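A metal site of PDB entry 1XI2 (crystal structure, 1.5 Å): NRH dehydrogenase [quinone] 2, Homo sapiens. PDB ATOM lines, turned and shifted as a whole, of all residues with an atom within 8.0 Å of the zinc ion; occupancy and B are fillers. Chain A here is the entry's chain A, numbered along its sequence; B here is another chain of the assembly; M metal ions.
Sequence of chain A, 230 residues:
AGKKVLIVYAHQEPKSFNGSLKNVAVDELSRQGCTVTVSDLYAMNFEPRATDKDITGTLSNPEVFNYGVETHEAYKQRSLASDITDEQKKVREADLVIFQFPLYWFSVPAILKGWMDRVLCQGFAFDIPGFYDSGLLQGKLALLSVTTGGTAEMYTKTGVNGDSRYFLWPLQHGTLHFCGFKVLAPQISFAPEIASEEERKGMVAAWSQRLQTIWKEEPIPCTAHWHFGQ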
ATOM      1  N   TYR A 132      24.421  16.334 -28.792  1.00  0.00           N
ATOM      2  CA  TYR A 132      24.648  14.901 -28.671  1.00  0.00           C
ATOM      3  C   TYR A 132      25.298  14.638 -27.317  1.00  0.00           C
ATOM      4  O   TYR A 132      24.776  15.106 -26.299  1.00  0.00           O
ATOM      5  CB  TYR A 132      25.495  14.373 -29.838  1.00  0.00           C
ATOM      6  CG  TYR A 132      24.656  14.170 -31.090  1.00  0.00           C
ATOM      7  CD1 TYR A 132      23.490  13.393 -31.055  1.00  0.00           C
ATOM      8  CD2 TYR A 132      25.011  14.762 -32.303  1.00  0.00           C
ATOM      9  CE1 TYR A 132      22.699  13.225 -32.192  1.00  0.00           C
ATOM     10  CE2 TYR A 132      24.219  14.596 -33.448  1.00  0.00           C
ATOM     11  CZ  TYR A 132      23.067  13.830 -33.382  1.00  0.00           C
ATOM     12  OH  TYR A 132      22.270  13.686 -34.502  1.00  0.00           O
ATOM     13  N   ASP A 133      26.412  13.916 -27.270  1.00  0.00           N
ATOM     14  CA  ASP A 133      27.047  13.638 -25.990  1.00  0.00           C
ATOM     15  C   ASP A 133      27.288  14.892 -25.138  1.00  0.00           C
ATOM     16  O   ASP A 133      27.245  14.827 -23.905  1.00  0.00           O
ATOM     17  CB  ASP A 133      28.376  12.904 -26.213  1.00  0.00           C
ATOM     18  CG  ASP A 133      28.177  11.429 -26.480  1.00  0.00           C
ATOM     19  OD1 ASP A 133      27.343  11.091 -27.339  1.00  0.00           O
ATOM     20  OD2 ASP A 133      28.869  10.613 -25.841  1.00  0.00           O
ATOM     21  N   TRP A 169      14.340   6.523 -34.148  1.00  0.00           N
ATOM     22  CA  TRP A 169      15.521   7.298 -34.526  1.00  0.00           C
ATOM     23  C   TRP A 169      15.407   8.819 -34.435  1.00  0.00           C
ATOM     24  O   TRP A 169      16.200   9.464 -33.746  1.00  0.00           O
ATOM     25  CB  TRP A 169      15.967   6.902 -35.941  1.00  0.00           C
ATOM     26  CG  TRP A 169      17.193   7.624 -36.441  1.00  0.00           C
ATOM     27  CD1 TRP A 169      17.247   8.534 -37.457  1.00  0.00           C
ATOM     28  CD2 TRP A 169      18.545   7.437 -36.001  1.00  0.00           C
ATOM     29  NE1 TRP A 169      18.537   8.919 -37.682  1.00  0.00           N
ATOM     30  CE2 TRP A 169      19.368   8.264 -36.796  1.00  0.00           C
ATOM     31  CE3 TRP A 169      19.140   6.655 -34.999  1.00  0.00           C
ATOM     32  CZ2 TRP A 169      20.746   8.328 -36.641  1.00  0.00           C
ATOM     33  CZ3 TRP A 169      20.527   6.715 -34.847  1.00  0.00           C
ATOM     34  CH2 TRP A 169      21.311   7.543 -35.657  1.00  0.00           C
ATOM     35  N   LEU A 171      13.269  10.622 -32.851  1.00  0.00           N
ATOM     36  CA  LEU A 171      12.928  11.001 -31.485  1.00  0.00           C
ATOM     37  C   LEU A 171      14.049  10.766 -30.487  1.00  0.00           C
ATOM     38  O   LEU A 171      14.470  11.698 -29.806  1.00  0.00           O
ATOM     39  CB  LEU A 171      11.679  10.221 -31.047  1.00  0.00           C
ATOM     40  CG  LEU A 171      10.441  10.454 -31.906  1.00  0.00           C
ATOM     41  CD1 LEU A 171       9.344   9.505 -31.476  1.00  0.00           C
ATOM     42  CD2 LEU A 171       9.977  11.893 -31.788  1.00  0.00           C
ATOM     43  N   GLN A 172      14.532   9.539 -30.392  1.00  0.00           N
ATOM     44  CA  GLN A 172      15.591   9.231 -29.434  1.00  0.00           C
ATOM     45  C   GLN A 172      16.951   9.828 -29.784  1.00  0.00           C
ATOM     46  O   GLN A 172      17.611  10.407 -28.928  1.00  0.00           O
ATOM     47  CB  GLN A 172      15.734   7.713 -29.280  1.00  0.00           C
ATOM     48  CG  GLN A 172      14.471   7.007 -28.823  1.00  0.00           C
ATOM     49  CD  GLN A 172      14.712   5.557 -28.428  1.00  0.00           C
ATOM     50  OE1 GLN A 172      15.513   4.854 -29.050  1.00  0.00           O
ATOM     51  NE2 GLN A 172      13.995   5.101 -27.415  1.00  0.00           N
ATOM     52  N   HIS A 173      17.364   9.683 -31.043  1.00  0.00           N
ATOM     53  CA  HIS A 173      18.662  10.199 -31.466  1.00  0.00           C
ATOM     54  C   HIS A 173      18.630  11.645 -31.941  1.00  0.00           C
ATOM     55  O   HIS A 173      19.351  12.499 -31.423  1.00  0.00           O
ATOM     56  CB  HIS A 173      19.239   9.319 -32.587  1.00  0.00           C
ATOM     57  CG  HIS A 173      20.609   9.738 -33.022  1.00  0.00           C
ATOM     58  ND1 HIS A 173      21.739   9.436 -32.299  1.00  0.00           N
ATOM     59  CD2 HIS A 173      21.028  10.445 -34.092  1.00  0.00           C
ATOM     60  CE1 HIS A 173      22.800   9.943 -32.900  1.00  0.00           C
ATOM     61  NE2 HIS A 173      22.395  10.560 -33.997  1.00  0.00           N
ATOM     62  N   GLY A 174      17.781  11.909 -32.938  1.00  0.00           N
ATOM     63  CA  GLY A 174      17.681  13.243 -33.493  1.00  0.00           C
ATOM     64  C   GLY A 174      17.217  14.330 -32.545  1.00  0.00           C
ATOM     65  O   GLY A 174      17.555  15.506 -32.739  1.00  0.00           O
ATOM     66  N   THR A 175      16.453  13.959 -31.527  1.00  0.00           N
ATOM     67  CA  THR A 175      15.951  14.951 -30.577  1.00  0.00           C
ATOM     68  C   THR A 175      16.535  14.822 -29.172  1.00  0.00           C
ATOM     69  O   THR A 175      17.265  15.707 -28.730  1.00  0.00           O
ATOM     70  CB  THR A 175      14.413  14.881 -30.483  1.00  0.00           C
ATOM     71  OG1 THR A 175      13.857  14.980 -31.805  1.00  0.00           O
ATOM     72  CG2 THR A 175      13.873  16.028 -29.636  1.00  0.00           C
ATOM     73  N   LEU A 176      16.227  13.727 -28.487  1.00  0.00           N
ATOM     74  CA  LEU A 176      16.692  13.522 -27.115  1.00  0.00           C
ATOM     75  C   LEU A 176      18.210  13.459 -26.968  1.00  0.00           C
ATOM     76  O   LEU A 176      18.793  14.212 -26.185  1.00  0.00           O
ATOM     77  CB  LEU A 176      16.032  12.271 -26.524  1.00  0.00           C
ATOM     78  CG  LEU A 176      14.503  12.309 -26.479  1.00  0.00           C
ATOM     79  CD1 LEU A 176      13.971  10.985 -25.962  1.00  0.00           C
ATOM     80  CD2 LEU A 176      14.033  13.455 -25.589  1.00  0.00           C
ATOM     81  N   HIS A 177      18.861  12.558 -27.710  1.00  0.00           N
ATOM     82  CA  HIS A 177      20.308  12.453 -27.615  1.00  0.00           C
ATOM     83  C   HIS A 177      20.968  13.762 -28.058  1.00  0.00           C
ATOM     84  O   HIS A 177      21.937  14.212 -27.449  1.00  0.00           O
ATOM     85  CB  HIS A 177      20.837  11.289 -28.464  1.00  0.00           C
ATOM     86  CG  HIS A 177      22.293  11.015 -28.296  1.00  0.00           C
ATOM     87  ND1 HIS A 177      22.945   9.982 -28.944  1.00  0.00           N
ATOM     88  CD2 HIS A 177      23.237  11.634 -27.551  1.00  0.00           C
ATOM     89  CE1 HIS A 177      24.215   9.975 -28.606  1.00  0.00           C
ATOM     90  NE2 HIS A 177      24.429  10.968 -27.771  1.00  0.00           N
ATOM     91  N   PHE A 178      20.442  14.371 -29.109  1.00  0.00           N
ATOM     92  CA  PHE A 178      21.007  15.616 -29.607  1.00  0.00           C
ATOM     93  C   PHE A 178      21.070  16.651 -28.493  1.00  0.00           C
ATOM     94  O   PHE A 178      22.002  17.443 -28.431  1.00  0.00           O
ATOM     95  CB  PHE A 178      20.153  16.164 -30.764  1.00  0.00           C
ATOM     96  CG  PHE A 178      20.801  17.302 -31.484  1.00  0.00           C
ATOM     97  CD1 PHE A 178      21.682  17.063 -32.537  1.00  0.00           C
ATOM     98  CD2 PHE A 178      20.558  18.620 -31.113  1.00  0.00           C
ATOM     99  CE1 PHE A 178      22.309  18.109 -33.192  1.00  0.00           C
ATOM    100  CE2 PHE A 178      21.181  19.680 -31.765  1.00  0.00           C
ATOM    101  CZ  PHE A 178      22.058  19.430 -32.809  1.00  0.00           C
ATOM    102  N   PHE A 181      20.395  14.194 -23.595  1.00  0.00           N
ATOM    103  CA  PHE A 181      19.676  13.213 -22.798  1.00  0.00           C
ATOM    104  C   PHE A 181      20.279  11.809 -22.905  1.00  0.00           C
ATOM    105  O   PHE A 181      20.720  11.382 -23.964  1.00  0.00           O
ATOM    106  CB  PHE A 181      18.217  13.104 -23.262  1.00  0.00           C
ATOM    107  CG  PHE A 181      17.312  14.173 -22.727  1.00  0.00           C
ATOM    108  CD1 PHE A 181      16.942  14.188 -21.391  1.00  0.00           C
ATOM    109  CD2 PHE A 181      16.779  15.130 -23.582  1.00  0.00           C
ATOM    110  CE1 PHE A 181      16.049  15.131 -20.907  1.00  0.00           C
ATOM    111  CE2 PHE A 181      15.875  16.079 -23.106  1.00  0.00           C
ATOM    112  CZ  PHE A 181      15.502  16.083 -21.762  1.00  0.00           C
ATOM    113  N   VAL A 183      19.262   8.198 -22.974  1.00  0.00           N
ATOM    114  CA  VAL A 183      17.994   7.564 -23.317  1.00  0.00           C
ATOM    115  C   VAL A 183      17.740   6.185 -22.737  1.00  0.00           C
ATOM    116  O   VAL A 183      18.440   5.235 -23.051  1.00  0.00           O
ATOM    117  CB  VAL A 183      17.842   7.474 -24.851  1.00  0.00           C
ATOM    118  CG1 VAL A 183      16.452   6.948 -25.215  1.00  0.00           C
ATOM    119  CG2 VAL A 183      18.076   8.836 -25.474  1.00  0.00           C
ATOM    120  N   ILE A 220      20.378   3.287 -22.986  1.00  0.00           N
ATOM    121  CA  ILE A 220      20.667   2.451 -24.142  1.00  0.00           C
ATOM    122  C   ILE A 220      21.763   3.146 -24.952  1.00  0.00           C
ATOM    123  O   ILE A 220      21.958   4.353 -24.819  1.00  0.00           O
ATOM    124  CB  ILE A 220      19.445   2.289 -25.064  1.00  0.00           C
ATOM    125  CG1 ILE A 220      19.083   3.647 -25.692  1.00  0.00           C
ATOM    126  CG2 ILE A 220      18.272   1.726 -24.285  1.00  0.00           C
ATOM    127  CD1 ILE A 220      18.007   3.562 -26.751  1.00  0.00           C
ATOM    128  N   PRO A 221      22.500   2.393 -25.764  1.00  0.00           N
ATOM    129  CA  PRO A 221      23.547   3.032 -26.560  1.00  0.00           C
ATOM    130  C   PRO A 221      22.835   3.667 -27.757  1.00  0.00           C
ATOM    131  O   PRO A 221      22.619   3.021 -28.780  1.00  0.00           O
ATOM    132  CB  PRO A 221      24.440   1.856 -26.963  1.00  0.00           C
ATOM    133  CG  PRO A 221      23.449   0.740 -27.125  1.00  0.00           C
ATOM    134  CD  PRO A 221      22.533   0.930 -25.924  1.00  0.00           C
ATOM    135  N   CYS A 222      22.446   4.930 -27.607  1.00  0.00           N
ATOM    136  CA  CYS A 222      21.731   5.628 -28.674  1.00  0.00           C
ATOM    137  C   CYS A 222      22.632   5.869 -29.886  1.00  0.00           C
ATOM    138  O   CYS A 222      23.146   6.970 -30.100  1.00  0.00           O
ATOM    139  CB  CYS A 222      21.185   6.957 -28.147  1.00  0.00           C
ATOM    140  SG  CYS A 222      19.885   7.667 -29.207  1.00  0.00           S
ATOM    141  N   THR A 223      22.797   4.826 -30.680  1.00  0.00           N
ATOM    142  CA  THR A 223      23.637   4.901 -31.871  1.00  0.00           C
ATOM    143  C   THR A 223      22.875   4.366 -33.076  1.00  0.00           C
ATOM    144  O   THR A 223      21.805   3.763 -32.941  1.00  0.00           O
ATOM    145  CB  THR A 223      24.905   4.058 -31.697  1.00  0.00           C
ATOM    146  OG1 THR A 223      24.543   2.693 -31.472  1.00  0.00           O
ATOM    147  CG2 THR A 223      25.714   4.557 -30.506  1.00  0.00           C
ATOM    148  N   ALA A 224      23.430   4.583 -34.269  1.00  0.00           N
ATOM    149  CA  ALA A 224      22.807   4.098 -35.491  1.00  0.00           C
ATOM    150  C   ALA A 224      22.747   2.573 -35.436  1.00  0.00           C
ATOM    151  O   ALA A 224      21.809   1.960 -35.942  1.00  0.00           O
ATOM    152  CB  ALA A 224      23.610   4.547 -36.703  1.00  0.00           C
ATOM    153  N   TRP A 226      22.363   0.586 -32.733  1.00  0.00           N
ATOM    154  CA  TRP A 226      21.247   0.167 -31.897  1.00  0.00           C
ATOM    155  C   TRP A 226      19.932   0.232 -32.661  1.00  0.00           C
ATOM    156  O   TRP A 226      19.126  -0.687 -32.604  1.00  0.00           O
ATOM    157  CB  TRP A 226      21.163   1.055 -30.643  1.00  0.00           C
ATOM    158  CG  TRP A 226      20.173   0.571 -29.631  1.00  0.00           C
ATOM    159  CD1 TRP A 226      20.407  -0.310 -28.605  1.00  0.00           C
ATOM    160  CD2 TRP A 226      18.775   0.901 -29.556  1.00  0.00           C
ATOM    161  NE1 TRP A 226      19.247  -0.530 -27.903  1.00  0.00           N
ATOM    162  CE2 TRP A 226      18.232   0.193 -28.470  1.00  0.00           C
ATOM    163  CE3 TRP A 226      17.945   1.735 -30.318  1.00  0.00           C
ATOM    164  CZ2 TRP A 226      16.884   0.287 -28.114  1.00  0.00           C
ATOM    165  CZ3 TRP A 226      16.596   1.829 -29.963  1.00  0.00           C
ATOM    166  CH2 TRP A 226      16.085   1.114 -28.872  1.00  0.00           C
ATOM    167  N   HIS A 227      19.718   1.341 -33.367  1.00  0.00           N
ATOM    168  CA  HIS A 227      18.485   1.532 -34.123  1.00  0.00           C
ATOM    169  C   HIS A 227      18.380   0.748 -35.421  1.00  0.00           C
ATOM    170  O   HIS A 227      17.308   0.271 -35.785  1.00  0.00           O
ATOM    171  CB  HIS A 227      18.268   3.014 -34.441  1.00  0.00           C
ATOM    172  CG  HIS A 227      18.004   3.875 -33.242  1.00  0.00           C
ATOM    173  ND1 HIS A 227      19.004   4.280 -32.378  1.00  0.00           N
ATOM    174  CD2 HIS A 227      16.855   4.404 -32.749  1.00  0.00           C
ATOM    175  CE1 HIS A 227      18.486   5.024 -31.422  1.00  0.00           C
ATOM    176  NE2 HIS A 227      17.187   5.108 -31.624  1.00  0.00           N
ATOM    177  N   VAL B 160      27.499  12.234 -37.975  1.00  0.00           N
ATOM    178  CA  VAL B 160      26.947  12.294 -36.625  1.00  0.00           C
ATOM    179  C   VAL B 160      25.422  12.192 -36.593  1.00  0.00           C
ATOM    180  O   VAL B 160      24.842  11.765 -35.601  1.00  0.00           O
ATOM    181  CB  VAL B 160      27.396  13.590 -35.915  1.00  0.00           C
ATOM    182  CG1 VAL B 160      26.721  14.803 -36.547  1.00  0.00           C
ATOM    183  CG2 VAL B 160      27.111  13.499 -34.439  1.00  0.00           C
HETATM  184 ZN    ZN M   1      21.760   8.672 -30.265  1.00  0.00          ZN
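The side-chain hydroxyl (OH) of Tyr 132 is in hydrogen-bond range of a ring nitrogen (NE2) of His 173 (3.2 Å).
The backbone carbonyl oxygen of His 173 lies within hydrogen-bond range of the backbone NH of Phe 178 (3.2 Å).
NE2 of His 173 sits at hydrogen-bond distance from O of Val 160 of chain B.
The backbone carbonyl oxygen (O) of Gln 172 sits close to the side-chain sulfur (SG) of Cys 222 (3.6 Å).
The backbone carbonyl oxygen (O) of Gln 172 is in hydrogen-bond range of the backbone NH (N) of His 177, at 2.8 Å.
NE2 of His 177 sits at hydrogen-bond distance from OD1 of Asp 133.
Within 4 Å of the zinc ion: His 173, His 177 and Cys 222.
The nearest printed residue that does not touch the zinc ion is Thr 223 (4.005 Å).
ND1 of His 173 binds the zinc ion, 2.2 Å away.
O of Cys 222 is bound to the zinc ion (2.2 Å).
A ring nitrogen (ND1) of His 177 is bound to the zinc ion, at 2.2 Å.
SG of Cys 222 is bound to the zinc ion (2.4 Å).
The zinc ion has four donor atoms within binding distance.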
